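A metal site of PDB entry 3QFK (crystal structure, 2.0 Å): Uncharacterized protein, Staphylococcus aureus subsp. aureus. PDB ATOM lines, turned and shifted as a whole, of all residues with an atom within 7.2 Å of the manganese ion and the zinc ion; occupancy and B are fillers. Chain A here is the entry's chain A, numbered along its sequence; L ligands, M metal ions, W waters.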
ATOM      1  N   SER A  26     -15.371 -26.291  17.295  1.00  0.00           N
ATOM      2  CA  SER A  26     -14.029 -26.376  16.767  1.00  0.00           C
ATOM      3  C   SER A  26     -13.376 -25.027  16.807  1.00  0.00           C
ATOM      4  O   SER A  26     -14.039 -23.997  16.788  1.00  0.00           O
ATOM      5  CB  SER A  26     -14.054 -26.877  15.319  1.00  0.00           C
ATOM      6  OG  SER A  26     -12.731 -27.067  14.834  1.00  0.00           O
ATOM      7  N   ASP A  27     -12.064 -25.035  16.886  1.00  0.00           N
ATOM      8  CA  ASP A  27     -11.294 -23.822  16.877  1.00  0.00           C
ATOM      9  C   ASP A  27     -11.801 -22.755  17.852  1.00  0.00           C
ATOM     10  O   ASP A  27     -11.935 -21.576  17.501  1.00  0.00           O
ATOM     11  CB  ASP A  27     -11.225 -23.271  15.451  1.00  0.00           C
ATOM     12  CG  ASP A  27     -10.556 -24.227  14.494  1.00  0.00           C
ATOM     13  OD1 ASP A  27      -9.347 -24.075  14.292  1.00  0.00           O
ATOM     14  OD2 ASP A  27     -11.227 -25.132  13.952  1.00  0.00           O
ATOM     15  N   VAL A  28     -12.112 -23.189  19.066  1.00  0.00           N
ATOM     16  CA  VAL A  28     -12.555 -22.315  20.118  1.00  0.00           C
ATOM     17  C   VAL A  28     -11.472 -21.315  20.486  1.00  0.00           C
ATOM     18  O   VAL A  28     -11.756 -20.159  20.815  1.00  0.00           O
ATOM     19  CB  VAL A  28     -13.029 -23.110  21.337  1.00  0.00           C
ATOM     20  CG1 VAL A  28     -13.385 -22.171  22.474  1.00  0.00           C
ATOM     21  CG2 VAL A  28     -14.208 -23.971  20.909  1.00  0.00           C
ATOM     22  N   HIS A  29     -10.229 -21.781  20.413  1.00  0.00           N
ATOM     23  CA  HIS A  29      -9.062 -20.934  20.599  1.00  0.00           C
ATOM     24  C   HIS A  29      -8.957 -20.178  21.943  1.00  0.00           C
ATOM     25  O   HIS A  29      -8.398 -19.093  22.007  1.00  0.00           O
ATOM     26  CB  HIS A  29      -8.930 -19.940  19.414  1.00  0.00           C
ATOM     27  CG  HIS A  29      -8.303 -20.538  18.180  1.00  0.00           C
ATOM     28  ND1 HIS A  29      -6.974 -20.922  18.152  1.00  0.00           N
ATOM     29  CD2 HIS A  29      -8.801 -20.807  16.949  1.00  0.00           C
ATOM     30  CE1 HIS A  29      -6.689 -21.415  16.956  1.00  0.00           C
ATOM     31  NE2 HIS A  29      -7.789 -21.359  16.209  1.00  0.00           N
ATOM     32  N   ASN A  70     -13.164 -30.146  18.314  1.00  0.00           N
ATOM     33  CA  ASN A  70     -12.332 -30.557  17.173  1.00  0.00           C
ATOM     34  C   ASN A  70     -10.982 -29.854  16.978  1.00  0.00           C
ATOM     35  O   ASN A  70     -10.531 -29.663  15.838  1.00  0.00           O
ATOM     36  CB  ASN A  70     -13.189 -30.503  15.904  1.00  0.00           C
ATOM     37  CG  ASN A  70     -12.551 -31.247  14.730  1.00  0.00           C
ATOM     38  OD1 ASN A  70     -11.942 -32.319  14.888  1.00  0.00           O
ATOM     39  ND2 ASN A  70     -12.697 -30.672  13.527  1.00  0.00           N
ATOM     40  N   GLY A  71     -10.314 -29.485  18.075  1.00  0.00           N
ATOM     41  CA  GLY A  71      -8.968 -28.917  17.982  1.00  0.00           C
ATOM     42  C   GLY A  71      -8.810 -27.406  18.005  1.00  0.00           C
ATOM     43  O   GLY A  71      -9.775 -26.672  17.805  1.00  0.00           O
ATOM     44  N   ASP A  72      -7.569 -26.965  18.194  1.00  0.00           N
ATOM     45  CA  ASP A  72      -7.256 -25.542  18.330  1.00  0.00           C
ATOM     46  C   ASP A  72      -8.003 -24.958  19.533  1.00  0.00           C
ATOM     47  O   ASP A  72      -8.685 -23.944  19.412  1.00  0.00           O
ATOM     48  CB  ASP A  72      -7.510 -24.777  17.029  1.00  0.00           C
ATOM     49  CG  ASP A  72      -6.337 -24.848  16.091  1.00  0.00           C
ATOM     50  OD1 ASP A  72      -5.392 -25.596  16.380  1.00  0.00           O
ATOM     51  OD2 ASP A  72      -6.318 -24.125  15.098  1.00  0.00           O
ATOM     52  N   PHE A  73      -7.842 -25.620  20.681  1.00  0.00           N
ATOM     53  CA  PHE A  73      -8.497 -25.209  21.922  1.00  0.00           C
ATOM     54  C   PHE A  73      -7.525 -24.634  22.962  1.00  0.00           C
ATOM     55  O   PHE A  73      -7.944 -23.971  23.910  1.00  0.00           O
ATOM     56  CB  PHE A  73      -9.234 -26.426  22.552  1.00  0.00           C
ATOM     57  CG  PHE A  73      -8.319 -27.531  23.037  1.00  0.00           C
ATOM     58  CD1 PHE A  73      -7.746 -27.487  24.302  1.00  0.00           C
ATOM     59  CD2 PHE A  73      -8.018 -28.603  22.212  1.00  0.00           C
ATOM     60  CE1 PHE A  73      -6.901 -28.517  24.753  1.00  0.00           C
ATOM     61  CE2 PHE A  73      -7.179 -29.640  22.652  1.00  0.00           C
ATOM     62  CZ  PHE A  73      -6.601 -29.574  23.919  1.00  0.00           C
ATOM     63  N   GLN A  75      -4.692 -22.493  22.484  1.00  0.00           N
ATOM     64  CA  GLN A  75      -4.052 -21.228  22.178  1.00  0.00           C
ATOM     65  C   GLN A  75      -4.941 -20.343  21.307  1.00  0.00           C
ATOM     66  O   GLN A  75      -5.757 -20.832  20.543  1.00  0.00           O
ATOM     67  CB  GLN A  75      -2.736 -21.512  21.416  1.00  0.00           C
ATOM     68  CG  GLN A  75      -1.916 -20.273  20.968  1.00  0.00           C
ATOM     69  CD  GLN A  75      -2.425 -19.593  19.692  1.00  0.00           C
ATOM     70  OE1 GLN A  75      -3.148 -20.187  18.910  1.00  0.00           O
ATOM     71  NE2 GLN A  75      -2.018 -18.360  19.484  1.00  0.00           N
ATOM     72  N   LEU A 107      -6.731 -33.097  18.177  1.00  0.00           N
ATOM     73  CA  LEU A 107      -5.657 -32.152  18.281  1.00  0.00           C
ATOM     74  C   LEU A 107      -5.623 -31.257  17.078  1.00  0.00           C
ATOM     75  O   LEU A 107      -5.651 -31.736  15.933  1.00  0.00           O
ATOM     76  CB  LEU A 107      -4.303 -32.866  18.341  1.00  0.00           C
ATOM     77  CG  LEU A 107      -3.974 -33.693  19.587  1.00  0.00           C
ATOM     78  CD1 LEU A 107      -2.651 -34.440  19.355  1.00  0.00           C
ATOM     79  CD2 LEU A 107      -3.902 -32.780  20.782  1.00  0.00           C
ATOM     80  N   GLY A 108      -5.528 -29.958  17.327  1.00  0.00           N
ATOM     81  CA  GLY A 108      -5.344 -28.988  16.240  1.00  0.00           C
ATOM     82  C   GLY A 108      -3.863 -28.603  16.174  1.00  0.00           C
ATOM     83  O   GLY A 108      -3.101 -28.973  17.061  1.00  0.00           O
ATOM     84  N   ASN A 109      -3.432 -27.900  15.109  1.00  0.00           N
ATOM     85  CA  ASN A 109      -2.031 -27.484  15.016  1.00  0.00           C
ATOM     86  C   ASN A 109      -1.583 -26.575  16.180  1.00  0.00           C
ATOM     87  O   ASN A 109      -0.431 -26.641  16.615  1.00  0.00           O
ATOM     88  CB  ASN A 109      -1.698 -26.784  13.680  1.00  0.00           C
ATOM     89  CG  ASN A 109      -2.658 -25.651  13.357  1.00  0.00           C
ATOM     90  OD1 ASN A 109      -3.882 -25.863  13.283  1.00  0.00           O
ATOM     91  ND2 ASN A 109      -2.121 -24.448  13.137  1.00  0.00           N
ATOM     92  N   HIS A 110      -2.488 -25.742  16.678  1.00  0.00           N
ATOM     93  CA  HIS A 110      -2.139 -24.835  17.762  1.00  0.00           C
ATOM     94  C   HIS A 110      -1.894 -25.492  19.130  1.00  0.00           C
ATOM     95  O   HIS A 110      -1.296 -24.850  19.995  1.00  0.00           O
ATOM     96  CB  HIS A 110      -3.078 -23.628  17.835  1.00  0.00           C
ATOM     97  CG  HIS A 110      -2.926 -22.704  16.664  1.00  0.00           C
ATOM     98  ND1 HIS A 110      -1.875 -21.817  16.553  1.00  0.00           N
ATOM     99  CD2 HIS A 110      -3.663 -22.565  15.532  1.00  0.00           C
ATOM    100  CE1 HIS A 110      -1.979 -21.151  15.416  1.00  0.00           C
ATOM    101  NE2 HIS A 110      -3.048 -21.590  14.766  1.00  0.00           N
ATOM    102  N   THR A 164      -4.255 -32.236  10.696  1.00  0.00           N
ATOM    103  CA  THR A 164      -3.485 -31.776   9.524  1.00  0.00           C
ATOM    104  C   THR A 164      -2.000 -32.173   9.666  1.00  0.00           C
ATOM    105  O   THR A 164      -1.370 -31.953  10.722  1.00  0.00           O
ATOM    106  CB  THR A 164      -3.648 -30.234   9.248  1.00  0.00           C
ATOM    107  OG1 THR A 164      -2.774 -29.829   8.172  1.00  0.00           O
ATOM    108  CG2 THR A 164      -3.330 -29.392  10.517  1.00  0.00           C
ATOM    109  N   TRP A 170       4.996 -25.125  10.238  1.00  0.00           N
ATOM    110  CA  TRP A 170       4.579 -24.020  11.075  1.00  0.00           C
ATOM    111  C   TRP A 170       5.229 -23.891  12.446  1.00  0.00           C
ATOM    112  O   TRP A 170       5.488 -22.787  12.922  1.00  0.00           O
ATOM    113  CB  TRP A 170       3.055 -24.144  11.329  1.00  0.00           C
ATOM    114  CG  TRP A 170       2.230 -24.222  10.051  1.00  0.00           C
ATOM    115  CD1 TRP A 170       2.443 -23.521   8.886  1.00  0.00           C
ATOM    116  CD2 TRP A 170       0.995 -24.919   9.875  1.00  0.00           C
ATOM    117  NE1 TRP A 170       1.463 -23.820   7.964  1.00  0.00           N
ATOM    118  CE2 TRP A 170       0.555 -24.664   8.549  1.00  0.00           C
ATOM    119  CE3 TRP A 170       0.236 -25.773  10.689  1.00  0.00           C
ATOM    120  CZ2 TRP A 170      -0.620 -25.206   8.043  1.00  0.00           C
ATOM    121  CZ3 TRP A 170      -0.916 -26.334  10.171  1.00  0.00           C
ATOM    122  CH2 TRP A 170      -1.330 -26.050   8.858  1.00  0.00           C
ATOM    123  N   HIS A 207      -9.073 -32.388  12.134  1.00  0.00           N
ATOM    124  CA  HIS A 207      -8.713 -31.021  12.316  1.00  0.00           C
ATOM    125  C   HIS A 207      -7.955 -30.584  11.052  1.00  0.00           C
ATOM    126  O   HIS A 207      -6.718 -30.533  11.015  1.00  0.00           O
ATOM    127  CB  HIS A 207      -7.847 -30.736  13.518  1.00  0.00           C
ATOM    128  CG  HIS A 207      -7.686 -29.280  13.737  1.00  0.00           C
ATOM    129  ND1 HIS A 207      -8.635 -28.526  14.400  1.00  0.00           N
ATOM    130  CD2 HIS A 207      -6.789 -28.393  13.235  1.00  0.00           C
ATOM    131  CE1 HIS A 207      -8.275 -27.251  14.366  1.00  0.00           C
ATOM    132  NE2 HIS A 207      -7.159 -27.143  13.661  1.00  0.00           N
ATOM    133  N   GLY A 208      -8.739 -30.383  10.004  1.00  0.00           N
ATOM    134  CA  GLY A 208      -8.244 -29.943   8.711  1.00  0.00           C
ATOM    135  C   GLY A 208      -9.498 -29.647   7.920  1.00  0.00           C
ATOM    136  O   GLY A 208     -10.624 -29.965   8.361  1.00  0.00           O
ATOM    137  N   GLU A 226      -1.827 -29.774   3.133  1.00  0.00           N
ATOM    138  CA  GLU A 226      -2.242 -29.174   4.387  1.00  0.00           C
ATOM    139  C   GLU A 226      -3.663 -29.611   4.669  1.00  0.00           C
ATOM    140  O   GLU A 226      -3.983 -30.017   5.765  1.00  0.00           O
ATOM    141  CB  GLU A 226      -2.170 -27.651   4.350  1.00  0.00           C
ATOM    142  CG  GLU A 226      -2.746 -26.981   5.629  1.00  0.00           C
ATOM    143  CD  GLU A 226      -2.802 -25.465   5.542  1.00  0.00           C
ATOM    144  OE1 GLU A 226      -3.400 -24.855   6.445  1.00  0.00           O
ATOM    145  OE2 GLU A 226      -2.260 -24.900   4.557  1.00  0.00           O
ATOM    146  N   GLY A 246     -12.469 -28.817  10.666  1.00  0.00           N
ATOM    147  CA  GLY A 246     -12.138 -27.565  11.352  1.00  0.00           C
ATOM    148  C   GLY A 246     -10.972 -26.933  10.622  1.00  0.00           C
ATOM    149  O   GLY A 246     -10.870 -27.070   9.410  1.00  0.00           O
ATOM    150  N   HIS A 247     -10.121 -26.248  11.369  1.00  0.00           N
ATOM    151  CA  HIS A 247      -8.883 -25.640  10.868  1.00  0.00           C
ATOM    152  C   HIS A 247      -9.027 -24.389   9.981  1.00  0.00           C
ATOM    153  O   HIS A 247      -8.302 -23.428  10.176  1.00  0.00           O
ATOM    154  CB  HIS A 247      -8.030 -26.702  10.133  1.00  0.00           C
ATOM    155  CG  HIS A 247      -6.685 -26.189   9.696  1.00  0.00           C
ATOM    156  ND1 HIS A 247      -5.745 -25.750  10.597  1.00  0.00           N
ATOM    157  CD2 HIS A 247      -6.129 -26.068   8.461  1.00  0.00           C
ATOM    158  CE1 HIS A 247      -4.666 -25.364   9.940  1.00  0.00           C
ATOM    159  NE2 HIS A 247      -4.865 -25.554   8.645  1.00  0.00           N
ATOM    160  N   GLN A 248      -9.950 -24.419   9.037  1.00  0.00           N
ATOM    161  CA  GLN A 248     -10.138 -23.325   8.100  1.00  0.00           C
ATOM    162  C   GLN A 248     -11.070 -22.247   8.615  1.00  0.00           C
ATOM    163  O   GLN A 248     -11.205 -21.218   7.973  1.00  0.00           O
ATOM    164  CB  GLN A 248     -10.658 -23.860   6.781  1.00  0.00           C
ATOM    165  CG  GLN A 248      -9.628 -24.648   5.975  1.00  0.00           C
ATOM    166  CD  GLN A 248     -10.246 -25.193   4.695  1.00  0.00           C
ATOM    167  OE1 GLN A 248     -11.369 -25.709   4.711  1.00  0.00           O
ATOM    168  NE2 GLN A 248      -9.536 -25.054   3.591  1.00  0.00           N
ATOM    169  N   HIS A 249     -11.730 -22.483   9.752  1.00  0.00           N
ATOM    170  CA  HIS A 249     -12.612 -21.492  10.361  1.00  0.00           C
ATOM    171  C   HIS A 249     -13.820 -21.152   9.494  1.00  0.00           C
ATOM    172  O   HIS A 249     -14.382 -20.060   9.608  1.00  0.00           O
ATOM    173  CB  HIS A 249     -11.814 -20.204  10.649  1.00  0.00           C
ATOM    174  CG  HIS A 249     -10.720 -20.378  11.648  1.00  0.00           C
ATOM    175  ND1 HIS A 249     -10.062 -19.305  12.221  1.00  0.00           N
ATOM    176  CD2 HIS A 249     -10.231 -21.483  12.264  1.00  0.00           C
ATOM    177  CE1 HIS A 249      -9.158 -19.755  13.082  1.00  0.00           C
ATOM    178  NE2 HIS A 249      -9.253 -21.074  13.133  1.00  0.00           N
ATOM    179  N   GLY A 265     -17.062 -23.185  12.195  1.00  0.00           N
ATOM    180  CA  GLY A 265     -16.471 -21.874  12.424  1.00  0.00           C
ATOM    181  C   GLY A 265     -15.373 -21.827  13.438  1.00  0.00           C
ATOM    182  O   GLY A 265     -14.528 -22.740  13.526  1.00  0.00           O
ATOM    183  N   THR A 266     -15.396 -20.768  14.242  1.00  0.00           N
ATOM    184  CA  THR A 266     -14.390 -20.536  15.249  1.00  0.00           C
ATOM    185  C   THR A 266     -14.912 -19.637  16.373  1.00  0.00           C
ATOM    186  O   THR A 266     -15.897 -18.928  16.192  1.00  0.00           O
ATOM    187  CB  THR A 266     -13.127 -19.873  14.591  1.00  0.00           C
ATOM    188  OG1 THR A 266     -12.057 -19.732  15.552  1.00  0.00           O
ATOM    189  CG2 THR A 266     -13.482 -18.487  13.974  1.00  0.00           C
ATOM    190  N   LYS A 428     -10.270 -18.630   3.828  1.00  0.00           N
ATOM    191  CA  LYS A 428      -9.950 -18.084   5.158  1.00  0.00           C
ATOM    192  C   LYS A 428      -9.009 -16.875   4.998  1.00  0.00           C
ATOM    193  O   LYS A 428      -8.034 -16.963   4.280  1.00  0.00           O
ATOM    194  CB  LYS A 428      -9.275 -19.130   6.058  1.00  0.00           C
ATOM    195  CG  LYS A 428      -8.872 -18.565   7.419  1.00  0.00           C
ATOM    196  CD  LYS A 428      -8.137 -19.569   8.303  1.00  0.00           C
ATOM    197  CE  LYS A 428      -7.684 -18.911   9.600  1.00  0.00           C
ATOM    198  NZ  LYS A 428      -6.817 -19.788  10.441  1.00  0.00           N
HETATM  199  C1  LIG L   1      -2.561 -18.984  12.146  1.00  0.00           C
HETATM  200  O1  LIG L   1      -3.394 -18.055  12.250  1.00  0.00           O
HETATM  201  O2  LIG L   1      -2.936 -20.151  11.936  1.00  0.00           O
HETATM  202  C2  LIG L   1      -1.121 -18.723  12.282  1.00  0.00           C
HETATM  203  O3  LIG L   1      -0.388 -19.668  12.498  1.00  0.00           O
HETATM  204  C3  LIG L   1      -0.558 -17.314  12.177  1.00  0.00           C
HETATM  205  C4  LIG L   1       0.854 -17.282  11.576  1.00  0.00           C
HETATM  206  C5  LIG L   1       1.846 -16.598  12.494  1.00  0.00           C
HETATM  207  O4  LIG L   1       2.433 -15.573  12.112  1.00  0.00           O
HETATM  208  O5  LIG L   1       2.043 -17.092  13.623  1.00  0.00           O
HETATM  209 MN    MN M   1      -5.905 -25.207  12.989  1.00  0.00          MN
HETATM  210 ZN    ZN M   2      -7.765 -22.554  14.264  1.00  0.00          ZN
HETATM  211  O   HOH W   1      -4.314 -22.306  12.112  1.00  0.00           O
HETATM  212  O   HOH W   2      -6.870 -23.086  12.142  1.00  0.00           O
HETATM  213  O   HOH W   3      -5.949 -21.076  13.661  1.00  0.00           O
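An oxygen (O2) of the ligand sits at hydrogen-bond distance from a ring nitrogen (NE2) of His 110, 3.2 Å away.
The zinc ion is bound by OD1 of Asp 27 (2.2 Å), NE2 of His 29 (2.3 Å), OD2 of Asp 72 (2.3 Å), water W2 (2.4 Å), NE2 of His 249 (2.4 Å) and water W3 (2.4 Å).
The manganese ion is bound by the side-chain amide oxygen (OD1) of Asn 109, a ring nitrogen (NE2) of His 207, the side-chain carboxylate (OD2) of Asp 72, a ring nitrogen (ND1) of His 247 and water W2.
The manganese ion has five donor atoms within binding distance.
Water W1 lies within hydrogen-bond range of an oxygen (O2) of the ligand (2.6 Å), a ring nitrogen (NE2) of His 110 (3.0 Å) and the side-chain amide nitrogen of Asn 109 (3.2 Å).
Within 4 Å of the zinc ion: Asp 27, His 29, Asp 72 and His 249.
The nearest printed residue that does not touch the zinc ion is His 247 (4.2 Å).
The backbone NH (N) of Thr 164 sits at hydrogen-bond distance from the backbone carbonyl oxygen (O) of His 207 (3.0 Å).
The side-chain carboxylate (OD2) of Asp 27 is in hydrogen-bond range of the side-chain hydroxyl (OG) of Ser 26, at 2.6 Å.
O of Gln 75 sits at hydrogen-bond distance from ND1 of His 29 (2.7 Å).
The backbone NH (N) of Asp 27 lies within hydrogen-bond range of the backbone carbonyl oxygen (O) of Gly 71 (3.0 Å).
The side-chain amide nitrogen (ND2) of Asn 109 sits close to a ring nitrogen (NE2) of His 110 (3.4 Å).
The backbone NH (N) of His 247 lies within hydrogen-bond range of the side-chain carboxylate (OD2) of Asp 27, at 3.0 Å.
The backbone NH (N) of His 110 sits at hydrogen-bond distance from the side-chain carboxylate (OD1) of Asp 72 (2.9 Å).
O of Asp 27 sits at hydrogen-bond distance from OG1 of Thr 266, 2.7 Å away.
Within 4 Å of the manganese ion: Asp 27, Asp 72, Asn 109, His 207 and His 247.
The nearest printed residue that does not touch the manganese ion is His 110 (4.3 Å).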
